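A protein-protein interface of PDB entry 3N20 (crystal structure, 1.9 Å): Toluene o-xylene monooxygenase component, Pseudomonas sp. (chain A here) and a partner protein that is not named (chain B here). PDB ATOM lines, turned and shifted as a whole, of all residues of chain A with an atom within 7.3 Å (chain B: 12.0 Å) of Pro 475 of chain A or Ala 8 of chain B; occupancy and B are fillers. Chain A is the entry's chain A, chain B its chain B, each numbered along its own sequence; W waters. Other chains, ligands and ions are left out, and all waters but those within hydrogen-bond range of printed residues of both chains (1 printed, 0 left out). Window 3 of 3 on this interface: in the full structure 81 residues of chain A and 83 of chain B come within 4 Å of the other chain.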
ATOM      1  N   ARG A 153     -10.071  21.118   1.963  1.00  0.00           N
ATOM      2  CA  ARG A 153      -9.620  22.321   2.639  1.00  0.00           C
ATOM      3  C   ARG A 153      -8.268  22.745   2.065  1.00  0.00           C
ATOM      4  O   ARG A 153      -7.876  23.902   2.176  1.00  0.00           O
ATOM      5  CB  ARG A 153      -9.495  22.045   4.134  1.00  0.00           C
ATOM      6  CG  ARG A 153      -9.420  23.281   5.004  1.00  0.00           C
ATOM      7  CD  ARG A 153     -10.752  24.005   5.056  1.00  0.00           C
ATOM      8  NE  ARG A 153     -10.746  25.019   6.100  1.00  0.00           N
ATOM      9  CZ  ARG A 153     -11.463  24.952   7.215  1.00  0.00           C
ATOM     10  NH1 ARG A 153     -12.260  23.917   7.436  1.00  0.00           N
ATOM     11  NH2 ARG A 153     -11.364  25.916   8.117  1.00  0.00           N
ATOM     12  N   LYS A 154      -7.561  21.801   1.447  1.00  0.00           N
ATOM     13  CA  LYS A 154      -6.254  22.094   0.860  1.00  0.00           C
ATOM     14  C   LYS A 154      -6.306  23.212  -0.182  1.00  0.00           C
ATOM     15  O   LYS A 154      -5.334  23.950  -0.353  1.00  0.00           O
ATOM     16  CB  LYS A 154      -5.661  20.839   0.207  1.00  0.00           C
ATOM     17  CG  LYS A 154      -5.226  19.755   1.181  1.00  0.00           C
ATOM     18  CD  LYS A 154      -4.695  18.532   0.436  1.00  0.00           C
ATOM     19  CE  LYS A 154      -4.179  17.463   1.403  1.00  0.00           C
ATOM     20  NZ  LYS A 154      -5.271  16.940   2.265  1.00  0.00           N
ATOM     21  N   LEU A 468       3.209  22.254  14.413  1.00  0.00           N
ATOM     22  CA  LEU A 468       2.188  22.114  13.379  1.00  0.00           C
ATOM     23  C   LEU A 468       1.150  23.220  13.519  1.00  0.00           C
ATOM     24  O   LEU A 468       0.720  23.816  12.528  1.00  0.00           O
ATOM     25  CB  LEU A 468       1.510  20.746  13.482  1.00  0.00           C
ATOM     26  CG  LEU A 468       2.327  19.578  12.918  1.00  0.00           C
ATOM     27  CD1 LEU A 468       1.746  18.247  13.383  1.00  0.00           C
ATOM     28  CD2 LEU A 468       2.337  19.666  11.390  1.00  0.00           C
ATOM     29  N   LEU A 473      -1.239  24.181  10.513  1.00  0.00           N
ATOM     30  CA  LEU A 473      -1.587  22.892   9.915  1.00  0.00           C
ATOM     31  C   LEU A 473      -2.440  22.016  10.833  1.00  0.00           C
ATOM     32  O   LEU A 473      -2.167  21.887  12.027  1.00  0.00           O
ATOM     33  CB  LEU A 473      -0.315  22.135   9.524  1.00  0.00           C
ATOM     34  CG  LEU A 473       0.469  22.738   8.354  1.00  0.00           C
ATOM     35  CD1 LEU A 473       1.833  22.062   8.218  1.00  0.00           C
ATOM     36  CD2 LEU A 473      -0.348  22.579   7.078  1.00  0.00           C
ATOM     37  N   GLU A 474      -3.471  21.409  10.255  1.00  0.00           N
ATOM     38  CA  GLU A 474      -4.381  20.541  10.991  1.00  0.00           C
ATOM     39  C   GLU A 474      -4.780  19.369  10.106  1.00  0.00           C
ATOM     40  O   GLU A 474      -4.649  19.440   8.885  1.00  0.00           O
ATOM     41  CB  GLU A 474      -5.645  21.315  11.378  1.00  0.00           C
ATOM     42  CG  GLU A 474      -5.436  22.416  12.399  1.00  0.00           C
ATOM     43  CD  GLU A 474      -6.701  23.235  12.629  1.00  0.00           C
ATOM     44  OE1 GLU A 474      -6.917  24.231  11.900  1.00  0.00           O
ATOM     45  OE2 GLU A 474      -7.487  22.871  13.529  1.00  0.00           O
ATOM     46  N   PRO A 475      -5.254  18.265  10.710  1.00  0.00           N
ATOM     47  CA  PRO A 475      -5.659  17.120   9.889  1.00  0.00           C
ATOM     48  C   PRO A 475      -6.683  17.627   8.875  1.00  0.00           C
ATOM     49  O   PRO A 475      -7.561  18.428   9.210  1.00  0.00           O
ATOM     50  CB  PRO A 475      -6.268  16.161  10.911  1.00  0.00           C
ATOM     51  CG  PRO A 475      -5.442  16.424  12.133  1.00  0.00           C
ATOM     52  CD  PRO A 475      -5.354  17.943  12.146  1.00  0.00           C
ATOM     53  N   GLY A 476      -6.568  17.161   7.641  1.00  0.00           N
ATOM     54  CA  GLY A 476      -7.466  17.622   6.602  1.00  0.00           C
ATOM     55  C   GLY A 476      -6.611  18.259   5.522  1.00  0.00           C
ATOM     56  O   GLY A 476      -6.861  18.061   4.330  1.00  0.00           O
ATOM     57  N   VAL A 477      -5.600  19.027   5.932  1.00  0.00           N
ATOM     58  CA  VAL A 477      -4.710  19.654   4.962  1.00  0.00           C
ATOM     59  C   VAL A 477      -3.280  19.129   5.115  1.00  0.00           C
ATOM     60  O   VAL A 477      -2.481  19.228   4.188  1.00  0.00           O
ATOM     61  CB  VAL A 477      -4.721  21.216   5.058  1.00  0.00           C
ATOM     62  CG1 VAL A 477      -6.033  21.697   5.663  1.00  0.00           C
ATOM     63  CG2 VAL A 477      -3.531  21.721   5.835  1.00  0.00           C
ATOM     64  N   MET A 478      -2.963  18.572   6.281  1.00  0.00           N
ATOM     65  CA  MET A 478      -1.635  18.006   6.523  1.00  0.00           C
ATOM     66  C   MET A 478      -1.390  16.901   5.494  1.00  0.00           C
ATOM     67  O   MET A 478      -2.222  16.014   5.314  1.00  0.00           O
ATOM     68  CB  MET A 478      -1.549  17.433   7.938  1.00  0.00           C
ATOM     69  CG  MET A 478      -1.375  18.481   9.026  1.00  0.00           C
ATOM     70  SD  MET A 478      -1.738  17.816  10.667  1.00  0.00           S
ATOM     71  CE  MET A 478      -0.443  16.571  10.818  1.00  0.00           C
ATOM     72  N   ALA B   8     -10.998  15.925  11.269  1.00  0.00           N
ATOM     73  CA  ALA B   8     -10.326  16.575  10.105  1.00  0.00           C
ATOM     74  C   ALA B   8     -11.103  17.814   9.664  1.00  0.00           C
ATOM     75  O   ALA B   8     -12.331  17.872   9.804  1.00  0.00           O
ATOM     76  CB  ALA B   8     -10.220  15.586   8.951  1.00  0.00           C
ATOM     77  N   LEU B   9     -10.383  18.809   9.148  1.00  0.00           N
ATOM     78  CA  LEU B   9     -11.002  20.047   8.675  1.00  0.00           C
ATOM     79  C   LEU B   9     -11.891  19.755   7.467  1.00  0.00           C
ATOM     80  O   LEU B   9     -11.459  19.117   6.505  1.00  0.00           O
ATOM     81  CB  LEU B   9      -9.930  21.066   8.267  1.00  0.00           C
ATOM     82  CG  LEU B   9      -9.075  21.745   9.341  1.00  0.00           C
ATOM     83  CD1 LEU B   9      -7.959  22.539   8.672  1.00  0.00           C
ATOM     84  CD2 LEU B   9      -9.947  22.657  10.201  1.00  0.00           C
ATOM     85  N   LYS B  10     -13.132  20.223   7.518  1.00  0.00           N
ATOM     86  CA  LYS B  10     -14.061  20.005   6.418  1.00  0.00           C
ATOM     87  C   LYS B  10     -13.949  21.098   5.363  1.00  0.00           C
ATOM     88  O   LYS B  10     -13.638  22.248   5.670  1.00  0.00           O
ATOM     89  CB  LYS B  10     -15.500  19.972   6.932  1.00  0.00           C
ATOM     90  CG  LYS B  10     -15.834  18.778   7.799  1.00  0.00           C
ATOM     91  CD  LYS B  10     -16.965  19.109   8.755  1.00  0.00           C
ATOM     92  CE  LYS B  10     -16.581  20.295   9.643  1.00  0.00           C
ATOM     93  NZ  LYS B  10     -17.247  20.251  10.979  1.00  0.00           N
ATOM     94  N   PRO B  11     -14.197  20.742   4.095  1.00  0.00           N
ATOM     95  CA  PRO B  11     -14.127  21.717   3.006  1.00  0.00           C
ATOM     96  C   PRO B  11     -15.141  22.840   3.231  1.00  0.00           C
ATOM     97  O   PRO B  11     -16.245  22.603   3.731  1.00  0.00           O
ATOM     98  CB  PRO B  11     -14.456  20.877   1.776  1.00  0.00           C
ATOM     99  CG  PRO B  11     -13.888  19.538   2.133  1.00  0.00           C
ATOM    100  CD  PRO B  11     -14.332  19.373   3.567  1.00  0.00           C
ATOM    101  N   LEU B  12     -14.754  24.058   2.867  1.00  0.00           N
ATOM    102  CA  LEU B  12     -15.609  25.231   3.019  1.00  0.00           C
ATOM    103  C   LEU B  12     -16.326  25.555   1.707  1.00  0.00           C
ATOM    104  O   LEU B  12     -16.031  24.973   0.663  1.00  0.00           O
ATOM    105  CB  LEU B  12     -14.760  26.424   3.451  1.00  0.00           C
ATOM    106  CG  LEU B  12     -14.761  26.910   4.909  1.00  0.00           C
ATOM    107  CD1 LEU B  12     -15.206  25.817   5.865  1.00  0.00           C
ATOM    108  CD2 LEU B  12     -13.359  27.397   5.243  1.00  0.00           C
HETATM  109  O   HOH W   1     -10.678  18.950   3.796  1.00  0.00           O
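O of Pro 475 of chain A sits at hydrogen-bond distance from N of Leu 9 of chain B (2.8 Å).
The guanidinium group (NH1) of Arg 153 of chain A lies within hydrogen-bond range of the backbone carbonyl oxygen (O) of Lys 10 of chain B, at 2.8 Å.
Among the printed residues, merely in contact across the chains: Arg 153 of chain A with Leu 9 of chain B (3.8 Å), Arg 153 of chain A with Leu 12 of chain B (3.6 Å), Glu 474 of chain A with Leu 9 of chain B (3.8 Å), Pro 475 of chain A with Ala 8 of chain B (3.4 Å) and Val 477 of chain A with Leu 9 of chain B (3.7 Å).
Of the printed residues of chain B, Pro 475 of chain A touches Ala 8 (3.4 Å) and Leu 9 (2.8 Å).
Of chain A, only Pro 475 comes within 4 Å of Ala 8 of chain B.
Glu 474 of chain A touches just one residue of chain B: Leu 9 (3.8 Å).
No residue of chain B comes within 4 Å of Gly 476 of chain A.
Val 477 of chain A touches one residue of chain B.
Of the printed residues of chain A, Leu 9 of chain B touches Arg 153 (3.8 Å), Glu 474 (3.8 Å), Pro 475 (2.8 Å) and Val 477 (3.7 Å).
Of the printed residues of chain B, Arg 153 of chain A touches Leu 9, Lys 10 and Leu 12.
Of the printed residues of chain A, Leu 12 of chain B touches Arg 153 (3.6 Å).
Of the printed residues of chain A, Lys 10 of chain B touches Arg 153 (2.8 Å).
The nearest residue of chain B that does not touch Pro 475 of chain A is Lys 10 of chain B (6.1 Å).
The nearest printed residue of chain A that does not touch Leu 12 of chain B is Lys 154 of chain A (7.7 Å).
Hydrophobic or aromatic side chains of chain B that line the printed part of chain A: Ala 8, Leu 9 and Leu 12.
Hydrophobic or aromatic side chains of chain A that line the printed part of chain B: Val 477.
Among the printed residues, 7 pairs touch across the chains.
Among the printed residues, no Asp or Glu carboxylate lies within 4 Å of a Lys or Arg side-chain nitrogen of the other chain.
Water W1 lies within hydrogen-bond range of the backbone carbonyl oxygen (O) of Leu 9 of chain B (2.8 Å) and the backbone NH (N) of Arg 153 of chain A (2.9 Å).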
